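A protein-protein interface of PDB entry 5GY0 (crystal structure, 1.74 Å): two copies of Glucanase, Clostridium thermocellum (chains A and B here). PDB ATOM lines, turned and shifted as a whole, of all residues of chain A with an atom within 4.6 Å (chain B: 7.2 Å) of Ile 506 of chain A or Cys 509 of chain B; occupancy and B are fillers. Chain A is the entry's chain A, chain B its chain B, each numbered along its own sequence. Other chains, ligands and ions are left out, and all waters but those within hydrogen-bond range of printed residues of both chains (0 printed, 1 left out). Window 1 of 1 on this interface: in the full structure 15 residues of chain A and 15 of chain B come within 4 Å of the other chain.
The backbone carbonyl oxygen of Ile 506 of chain A sits close to the backbone carbonyl oxygen of Met 513 of chain B (3.5 Å). OG1 of Thr 505 of chain A lies within hydrogen-bond range of OD1 of Asp 514 of chain B (2.6 Å). The backbone carbonyl oxygen (O) of Gly 507 of chain A sits close to the backbone carbonyl oxygen (O) of Glu 510 of chain B (3.5 Å). SG of Cys 509 of chain A forms a disulfide with SG of Cys 509 of chain B. N of Tyr 508 of chain B lies close to SG of Cys 509 of chain A, at 3.7 Å. The backbone carbonyl oxygen of Ile 506 of chain A lies within hydrogen-bond range of the backbone NH of Val 515 of chain B (2.9 Å). The backbone NH (N) of Gly 512 of chain B sits at hydrogen-bond distance from the backbone carbonyl oxygen (O) of Gly 507 of chain A (2.9 Å).
O of Asp 514 of chain B sits at hydrogen-bond distance from N of Ile 535 of chain B, at 3.0 Å. The backbone NH (N) of Gln 553 of chain B lies within hydrogen-bond range of the backbone carbonyl oxygen (O) of Tyr 508 of chain B (2.8 Å). The side-chain carboxylate (OE1) of Glu 510 of chain B sits at hydrogen-bond distance from the backbone NH (N) of Glu 551 of chain B (3.0 Å). N of Gln 553 of chain A lies within hydrogen-bond range of O of Tyr 508 of chain A. The backbone NH (N) of Gly 507 of chain A sits at hydrogen-bond distance from the backbone carbonyl oxygen (O) of Gln 553 of chain A (2.8 Å).
Among the printed residues, merely in contact across the chains: Thr 505 of chain A with Val 515 of chain B (3.4 Å), Thr 505 of chain A with Glu 516 of chain B (3.9 Å), Thr 505 of chain A with Ile 535 of chain B (3.96 Å), Ile 506 of chain A with Ile 506 of chain B (3.9 Å), Ile 506 of chain A with Cys 509 of chain B (3.8 Å), Ile 506 of chain A with Asp 514 of chain B (3.4 Å), Gly 507 of chain A with Ser 511 of chain B (3.5 Å), Gly 507 of chain A with Met 513 of chain B (3.9 Å), Tyr 508 of chain A with Cys 509 of chain B (3.3 Å) and Tyr 508 of chain A with Ser 511 of chain B (3.6 Å).
Of chain B, only Ile 506 (3.9 Å), Cys 509 (3.8 Å), Met 513 (3.5 Å), Asp 514 (3.4 Å) and Val 515 (2.9 Å) come within 4 Å of Ile 506 of chain A. Of chain A, only Ile 506 (3.8 Å), Tyr 508 (3.3 Å) and Cys 509 (2.1 Å) come within 4 Å of Cys 509 of chain B. Printed residues of chain B within 4 Å of Tyr 508 of chain A: Cys 509 (3.3 Å) and Ser 511 (3.6 Å). Printed residues of chain A within 4 Å of Val 515 of chain B: Thr 505 and Ile 506. Of the printed residues of chain A, Glu 516 of chain B touches Thr 505 (3.9 Å). Tyr 534 of chain B touches none of the printed residues of chain A. Gly 507 of chain B touches none of the printed residues of chain A. The nearest residue of chain B that does not touch Ile 506 of chain A is Glu 516 of chain B (5.1 Å). The nearest printed residue of chain A that does not touch Cys 509 of chain B is Gly 507 of chain A (4.7 Å).
Of the 17 printed residues of chain B, 11 touch a printed residue of chain A. Hydrophobic or aromatic side chains of chain B within 4 Å of the printed part of chain A: Ile 506, Tyr 508, Val 515 and Ile 535. Of the 9 printed residues of chain A, 5 touch a printed residue of chain B. Hydrophobic or aromatic side chains of chain A that line the printed part of chain B: Ile 506 and Tyr 508. Among the printed residues, no Asp or Glu carboxylate lies within 4 Å of a Lys or Arg side-chain nitrogen of the other chain.
Ile 506 of chain B touches its own counterpart, Ile 506 of chain A. Ile 506 of chain A touches Cys 509 of chain B, but with the chains exchanged Cys 509 of chain A does not touch Ile 506 of chain B (4.02 Å). Tyr 508 of chain A touches Cys 509 of chain B, and with the chains exchanged Cys 509 of chain A touches Tyr 508 of chain B. Cys 509 of chain A touches its own counterpart, Cys 509 of chain B. Of the 17 pairs that touch across the chains among the printed residues, 4 have their exchanged pair printed and touching as well.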
ATOM      1  N   THR A 505       1.004 -17.770 -11.891  1.00  0.00           N
ATOM      2  CA  THR A 505       1.971 -16.747 -11.520  1.00  0.00           C
ATOM      3  C   THR A 505       2.754 -16.347 -12.775  1.00  0.00           C
ATOM      4  O   THR A 505       2.672 -17.004 -13.810  1.00  0.00           O
ATOM      5  CB  THR A 505       2.950 -17.271 -10.443  1.00  0.00           C
ATOM      6  OG1 THR A 505       3.572 -18.479 -10.906  1.00  0.00           O
ATOM      7  CG2 THR A 505       2.230 -17.577  -9.146  1.00  0.00           C
ATOM      8  N   ILE A 506       3.496 -15.249 -12.674  1.00  0.00           N
ATOM      9  CA  ILE A 506       4.277 -14.722 -13.785  1.00  0.00           C
ATOM     10  C   ILE A 506       5.751 -14.716 -13.387  1.00  0.00           C
ATOM     11  O   ILE A 506       6.120 -14.304 -12.281  1.00  0.00           O
ATOM     12  CB  ILE A 506       3.858 -13.261 -14.084  1.00  0.00           C
ATOM     13  CG1 ILE A 506       2.414 -13.193 -14.584  1.00  0.00           C
ATOM     14  CG2 ILE A 506       4.775 -12.622 -15.118  1.00  0.00           C
ATOM     15  CD1 ILE A 506       2.105 -14.203 -15.638  1.00  0.00           C
ATOM     16  N   GLY A 507       6.594 -15.163 -14.310  1.00  0.00           N
ATOM     17  CA  GLY A 507       8.022 -15.200 -14.055  1.00  0.00           C
ATOM     18  C   GLY A 507       8.793 -14.146 -14.828  1.00  0.00           C
ATOM     19  O   GLY A 507       9.953 -13.908 -14.539  1.00  0.00           O
ATOM     20  N   TYR A 508       8.165 -13.546 -15.835  1.00  0.00           N
ATOM     21  CA  TYR A 508       8.776 -12.458 -16.593  1.00  0.00           C
ATOM     22  C   TYR A 508       7.665 -11.849 -17.432  1.00  0.00           C
ATOM     23  O   TYR A 508       6.875 -12.566 -18.044  1.00  0.00           O
ATOM     24  CB  TYR A 508       9.864 -12.956 -17.549  1.00  0.00           C
ATOM     25  CG  TYR A 508      10.374 -11.875 -18.488  1.00  0.00           C
ATOM     26  CD1 TYR A 508      10.977 -10.705 -18.008  1.00  0.00           C
ATOM     27  CD2 TYR A 508      10.244 -12.024 -19.865  1.00  0.00           C
ATOM     28  CE1 TYR A 508      11.441  -9.716 -18.883  1.00  0.00           C
ATOM     29  CE2 TYR A 508      10.687 -11.044 -20.734  1.00  0.00           C
ATOM     30  CZ  TYR A 508      11.294  -9.905 -20.244  1.00  0.00           C
ATOM     31  OH  TYR A 508      11.750  -8.951 -21.124  1.00  0.00           O
ATOM     32  N   CYS A 509       7.615 -10.527 -17.465  1.00  0.00           N
ATOM     33  CA  CYS A 509       6.726  -9.898 -18.418  1.00  0.00           C
ATOM     34  C   CYS A 509       7.429  -8.687 -19.014  1.00  0.00           C
ATOM     35  O   CYS A 509       7.918  -7.792 -18.315  1.00  0.00           O
ATOM     36  CB  CYS A 509       5.348  -9.656 -17.794  1.00  0.00           C
ATOM     37  SG  CYS A 509       5.181  -8.206 -16.795  1.00  0.00           S
ATOM     38  N   ILE A 517      -3.814 -11.497 -17.372  1.00  0.00           N
ATOM     39  CA  ILE A 517      -4.032 -12.933 -17.485  1.00  0.00           C
ATOM     40  C   ILE A 517      -5.318 -13.238 -16.738  1.00  0.00           C
ATOM     41  O   ILE A 517      -5.490 -12.832 -15.583  1.00  0.00           O
ATOM     42  CB  ILE A 517      -2.877 -13.797 -16.927  1.00  0.00           C
ATOM     43  CG1 ILE A 517      -1.525 -13.354 -17.497  1.00  0.00           C
ATOM     44  CG2 ILE A 517      -3.127 -15.266 -17.264  1.00  0.00           C
ATOM     45  CD1 ILE A 517      -0.926 -12.139 -16.816  1.00  0.00           C
ATOM     46  N   LEU A 552       6.065 -13.298 -22.515  1.00  0.00           N
ATOM     47  CA  LEU A 552       5.530 -13.504 -21.173  1.00  0.00           C
ATOM     48  C   LEU A 552       6.011 -14.866 -20.725  1.00  0.00           C
ATOM     49  O   LEU A 552       5.949 -15.811 -21.502  1.00  0.00           O
ATOM     50  CB  LEU A 552       3.997 -13.513 -21.210  1.00  0.00           C
ATOM     51  CG  LEU A 552       3.259 -13.667 -19.872  1.00  0.00           C
ATOM     52  CD1 LEU A 552       3.515 -12.494 -18.946  1.00  0.00           C
ATOM     53  CD2 LEU A 552       1.750 -13.782 -20.108  1.00  0.00           C
ATOM     54  N   GLN A 553       6.432 -15.000 -19.469  1.00  0.00           N
ATOM     55  CA  GLN A 553       6.631 -16.333 -18.898  1.00  0.00           C
ATOM     56  C   GLN A 553       5.594 -16.556 -17.805  1.00  0.00           C
ATOM     57  O   GLN A 553       5.543 -15.775 -16.857  1.00  0.00           O
ATOM     58  CB  GLN A 553       8.047 -16.488 -18.338  1.00  0.00           C
ATOM     59  CG  GLN A 553       9.122 -16.413 -19.417  1.00  0.00           C
ATOM     60  CD  GLN A 553      10.530 -16.231 -18.870  1.00  0.00           C
ATOM     61  OE1 GLN A 553      10.836 -16.591 -17.727  1.00  0.00           O
ATOM     62  NE2 GLN A 553      11.409 -15.682 -19.708  1.00  0.00           N
ATOM     63  N   PHE A 554       4.750 -17.575 -17.961  1.00  0.00           N
ATOM     64  CA  PHE A 554       3.682 -17.797 -16.987  1.00  0.00           C
ATOM     65  C   PHE A 554       3.751 -19.211 -16.447  1.00  0.00           C
ATOM     66  O   PHE A 554       4.151 -20.142 -17.149  1.00  0.00           O
ATOM     67  CB  PHE A 554       2.287 -17.459 -17.542  1.00  0.00           C
ATOM     68  CG  PHE A 554       1.873 -18.263 -18.757  1.00  0.00           C
ATOM     69  CD1 PHE A 554       1.246 -19.494 -18.618  1.00  0.00           C
ATOM     70  CD2 PHE A 554       2.092 -17.763 -20.039  1.00  0.00           C
ATOM     71  CE1 PHE A 554       0.841 -20.225 -19.736  1.00  0.00           C
ATOM     72  CE2 PHE A 554       1.675 -18.471 -21.169  1.00  0.00           C
ATOM     73  CZ  PHE A 554       1.075 -19.718 -21.021  1.00  0.00           C
ATOM     74  N   ILE B 506      -0.205  -5.736 -15.711  1.00  0.00           N
ATOM     75  CA  ILE B 506       1.217  -5.592 -15.427  1.00  0.00           C
ATOM     76  C   ILE B 506       1.906  -5.061 -16.684  1.00  0.00           C
ATOM     77  O   ILE B 506       1.526  -5.432 -17.803  1.00  0.00           O
ATOM     78  CB  ILE B 506       1.835  -6.907 -14.912  1.00  0.00           C
ATOM     79  CG1 ILE B 506       1.316  -8.102 -15.707  1.00  0.00           C
ATOM     80  CG2 ILE B 506       1.472  -7.103 -13.442  1.00  0.00           C
ATOM     81  CD1 ILE B 506       1.530  -9.458 -15.040  1.00  0.00           C
ATOM     82  N   GLY B 507       2.865  -4.156 -16.488  1.00  0.00           N
ATOM     83  CA  GLY B 507       3.631  -3.563 -17.589  1.00  0.00           C
ATOM     84  C   GLY B 507       5.103  -3.951 -17.627  1.00  0.00           C
ATOM     85  O   GLY B 507       5.782  -3.732 -18.638  1.00  0.00           O
ATOM     86  N   TYR B 508       5.589  -4.551 -16.540  1.00  0.00           N
ATOM     87  CA  TYR B 508       6.953  -5.091 -16.469  1.00  0.00           C
ATOM     88  C   TYR B 508       7.053  -5.953 -15.215  1.00  0.00           C
ATOM     89  O   TYR B 508       6.582  -5.543 -14.162  1.00  0.00           O
ATOM     90  CB  TYR B 508       8.017  -3.988 -16.430  1.00  0.00           C
ATOM     91  CG  TYR B 508       9.412  -4.546 -16.220  1.00  0.00           C
ATOM     92  CD1 TYR B 508       9.997  -5.394 -17.151  1.00  0.00           C
ATOM     93  CD2 TYR B 508      10.124  -4.240 -15.062  1.00  0.00           C
ATOM     94  CE1 TYR B 508      11.264  -5.920 -16.934  1.00  0.00           C
ATOM     95  CE2 TYR B 508      11.389  -4.752 -14.843  1.00  0.00           C
ATOM     96  CZ  TYR B 508      11.954  -5.587 -15.783  1.00  0.00           C
ATOM     97  OH  TYR B 508      13.222  -6.080 -15.561  1.00  0.00           O
ATOM     98  N   CYS B 509       7.606  -7.151 -15.346  1.00  0.00           N
ATOM     99  CA  CYS B 509       7.757  -8.108 -14.236  1.00  0.00           C
ATOM    100  C   CYS B 509       9.184  -8.621 -14.404  1.00  0.00           C
ATOM    101  O   CYS B 509       9.469  -9.324 -15.368  1.00  0.00           O
ATOM    102  CB  CYS B 509       6.800  -9.308 -14.384  1.00  0.00           C
ATOM    103  SG  CYS B 509       5.103  -8.824 -14.834  1.00  0.00           S
ATOM    104  N   GLU B 510      10.085  -8.266 -13.493  1.00  0.00           N
ATOM    105  CA  GLU B 510      11.487  -8.652 -13.616  1.00  0.00           C
ATOM    106  C   GLU B 510      11.685 -10.162 -13.761  1.00  0.00           C
ATOM    107  O   GLU B 510      11.078 -10.955 -13.035  1.00  0.00           O
ATOM    108  CB  GLU B 510      12.272  -8.119 -12.409  1.00  0.00           C
ATOM    109  CG  GLU B 510      13.749  -8.506 -12.452  1.00  0.00           C
ATOM    110  CD  GLU B 510      14.508  -7.936 -11.264  1.00  0.00           C
ATOM    111  OE1 GLU B 510      13.884  -7.244 -10.438  1.00  0.00           O
ATOM    112  OE2 GLU B 510      15.734  -8.153 -11.164  1.00  0.00           O
ATOM    113  N   SER B 511      12.516 -10.542 -14.726  1.00  0.00           N
ATOM    114  CA  SER B 511      12.793 -11.949 -15.014  1.00  0.00           C
ATOM    115  C   SER B 511      13.272 -12.740 -13.796  1.00  0.00           C
ATOM    116  O   SER B 511      14.156 -12.298 -13.063  1.00  0.00           O
ATOM    117  CB  SER B 511      13.847 -12.038 -16.115  1.00  0.00           C
ATOM    118  OG  SER B 511      13.979 -13.379 -16.559  1.00  0.00           O
ATOM    119  N   GLY B 512      12.651 -13.892 -13.566  1.00  0.00           N
ATOM    120  CA  GLY B 512      13.114 -14.809 -12.533  1.00  0.00           C
ATOM    121  C   GLY B 512      12.490 -14.579 -11.173  1.00  0.00           C
ATOM    122  O   GLY B 512      12.768 -15.319 -10.232  1.00  0.00           O
ATOM    123  N   MET B 513      11.630 -13.572 -11.064  1.00  0.00           N
ATOM    124  CA  MET B 513      10.952 -13.268  -9.806  1.00  0.00           C
ATOM    125  C   MET B 513       9.497 -13.732  -9.899  1.00  0.00           C
ATOM    126  O   MET B 513       8.637 -12.962 -10.324  1.00  0.00           O
ATOM    127  CB  MET B 513      10.997 -11.762  -9.537  1.00  0.00           C
ATOM    128  CG  MET B 513      12.400 -11.206  -9.289  1.00  0.00           C
ATOM    129  SD  MET B 513      13.275 -12.015  -7.912  1.00  0.00           S
ATOM    130  CE  MET B 513      11.998 -12.163  -6.654  1.00  0.00           C
ATOM    131  N   ASP B 514       9.229 -14.980  -9.518  1.00  0.00           N
ATOM    132  CA  ASP B 514       7.899 -15.586  -9.670  1.00  0.00           C
ATOM    133  C   ASP B 514       6.966 -14.750  -8.802  1.00  0.00           C
ATOM    134  O   ASP B 514       7.167 -14.622  -7.590  1.00  0.00           O
ATOM    135  CB  ASP B 514       7.944 -17.052  -9.214  1.00  0.00           C
ATOM    136  CG  ASP B 514       6.661 -17.839  -9.523  1.00  0.00           C
ATOM    137  OD1 ASP B 514       6.052 -17.656 -10.605  1.00  0.00           O
ATOM    138  OD2 ASP B 514       6.308 -18.728  -8.711  1.00  0.00           O
ATOM    139  N   VAL B 515       5.951 -14.172  -9.431  1.00  0.00           N
ATOM    140  CA  VAL B 515       5.103 -13.197  -8.758  1.00  0.00           C
ATOM    141  C   VAL B 515       3.636 -13.437  -9.066  1.00  0.00           C
ATOM    142  O   VAL B 515       3.261 -13.883 -10.149  1.00  0.00           O
ATOM    143  CB  VAL B 515       5.526 -11.733  -9.087  1.00  0.00           C
ATOM    144  CG1 VAL B 515       5.313 -11.372 -10.557  1.00  0.00           C
ATOM    145  CG2 VAL B 515       4.859 -10.725  -8.167  1.00  0.00           C
ATOM    146  N   GLU B 516       2.810 -13.128  -8.072  1.00  0.00           N
ATOM    147  CA  GLU B 516       1.373 -13.066  -8.281  1.00  0.00           C
ATOM    148  C   GLU B 516       0.803 -11.779  -7.709  1.00  0.00           C
ATOM    149  O   GLU B 516       1.363 -11.181  -6.791  1.00  0.00           O
ATOM    150  CB  GLU B 516       0.672 -14.272  -7.650  1.00  0.00           C
ATOM    151  CG  GLU B 516       0.860 -14.406  -6.156  1.00  0.00           C
ATOM    152  CD  GLU B 516      -0.136 -15.374  -5.543  1.00  0.00           C
ATOM    153  OE1 GLU B 516      -1.170 -15.655  -6.186  1.00  0.00           O
ATOM    154  OE2 GLU B 516       0.123 -15.851  -4.420  1.00  0.00           O
ATOM    155  N   ILE B 517      -0.297 -11.320  -8.288  1.00  0.00           N
ATOM    156  CA  ILE B 517      -0.975 -10.154  -7.753  1.00  0.00           C
ATOM    157  C   ILE B 517      -2.391 -10.623  -7.435  1.00  0.00           C
ATOM    158  O   ILE B 517      -3.053 -11.225  -8.280  1.00  0.00           O
ATOM    159  CB  ILE B 517      -1.032  -8.993  -8.763  1.00  0.00           C
ATOM    160  CG1 ILE B 517       0.370  -8.614  -9.248  1.00  0.00           C
ATOM    161  CG2 ILE B 517      -1.741  -7.798  -8.139  1.00  0.00           C
ATOM    162  CD1 ILE B 517       0.350  -7.409 -10.182  1.00  0.00           C
ATOM    163  N   TYR B 534       5.663 -12.401  -3.769  1.00  0.00           N
ATOM    164  CA  TYR B 534       6.732 -13.148  -4.408  1.00  0.00           C
ATOM    165  C   TYR B 534       6.753 -14.573  -3.870  1.00  0.00           C
ATOM    166  O   TYR B 534       6.853 -14.773  -2.657  1.00  0.00           O
ATOM    167  CB  TYR B 534       8.075 -12.435  -4.217  1.00  0.00           C
ATOM    168  CG  TYR B 534       8.106 -11.210  -5.092  1.00  0.00           C
ATOM    169  CD1 TYR B 534       8.438 -11.326  -6.444  1.00  0.00           C
ATOM    170  CD2 TYR B 534       7.745  -9.962  -4.597  1.00  0.00           C
ATOM    171  CE1 TYR B 534       8.423 -10.223  -7.277  1.00  0.00           C
ATOM    172  CE2 TYR B 534       7.721  -8.839  -5.431  1.00  0.00           C
ATOM    173  CZ  TYR B 534       8.064  -8.990  -6.763  1.00  0.00           C
ATOM    174  OH  TYR B 534       8.057  -7.909  -7.616  1.00  0.00           O
ATOM    175  N   ILE B 535       6.604 -15.547  -4.764  1.00  0.00           N
ATOM    176  CA  ILE B 535       6.521 -16.941  -4.347  1.00  0.00           C
ATOM    177  C   ILE B 535       7.818 -17.465  -3.726  1.00  0.00           C
ATOM    178  O   ILE B 535       7.806 -18.244  -2.767  1.00  0.00           O
ATOM    179  CB  ILE B 535       6.071 -17.830  -5.516  1.00  0.00           C
ATOM    180  CG1 ILE B 535       4.784 -17.271  -6.141  1.00  0.00           C
ATOM    181  CG2 ILE B 535       5.925 -19.277  -5.052  1.00  0.00           C
ATOM    182  CD1 ILE B 535       3.674 -16.938  -5.159  1.00  0.00           C
ATOM    183  N   GLU B 551      11.657  -5.620  -9.248  1.00  0.00           N
ATOM    184  CA  GLU B 551      10.884  -4.570  -9.912  1.00  0.00           C
ATOM    185  C   GLU B 551       9.596  -5.128 -10.538  1.00  0.00           C
ATOM    186  O   GLU B 551       9.608  -6.112 -11.284  1.00  0.00           O
ATOM    187  CB  GLU B 551      11.732  -3.865 -10.981  1.00  0.00           C
ATOM    188  CG  GLU B 551      10.915  -2.760 -11.670  1.00  0.00           C
ATOM    189  CD  GLU B 551      11.735  -1.915 -12.626  1.00  0.00           C
ATOM    190  OE1 GLU B 551      12.982  -2.005 -12.614  1.00  0.00           O
ATOM    191  OE2 GLU B 551      11.127  -1.180 -13.428  1.00  0.00           O
ATOM    192  N   LEU B 552       8.480  -4.478 -10.227  1.00  0.00           N
ATOM    193  CA  LEU B 552       7.206  -4.767 -10.887  1.00  0.00           C
ATOM    194  C   LEU B 552       6.597  -3.422 -11.298  1.00  0.00           C
ATOM    195  O   LEU B 552       6.632  -2.454 -10.532  1.00  0.00           O
ATOM    196  CB  LEU B 552       6.254  -5.495  -9.928  1.00  0.00           C
ATOM    197  CG  LEU B 552       4.873  -5.884 -10.478  1.00  0.00           C
ATOM    198  CD1 LEU B 552       4.969  -6.927 -11.575  1.00  0.00           C
ATOM    199  CD2 LEU B 552       3.989  -6.442  -9.364  1.00  0.00           C
ATOM    200  N   GLN B 553       6.066  -3.360 -12.516  1.00  0.00           N
ATOM    201  CA  GLN B 553       5.230  -2.223 -12.911  1.00  0.00           C
ATOM    202  C   GLN B 553       3.795  -2.734 -13.033  1.00  0.00           C
ATOM    203  O   GLN B 553       3.524  -3.657 -13.810  1.00  0.00           O
ATOM    204  CB  GLN B 553       5.736  -1.620 -14.225  1.00  0.00           C
ATOM    205  CG  GLN B 553       7.105  -0.949 -14.073  1.00  0.00           C
ATOM    206  CD  GLN B 553       7.768  -0.630 -15.402  1.00  0.00           C
ATOM    207  OE1 GLN B 553       7.105  -0.461 -16.436  1.00  0.00           O
ATOM    208  NE2 GLN B 553       9.092  -0.546 -15.376  1.00  0.00           N
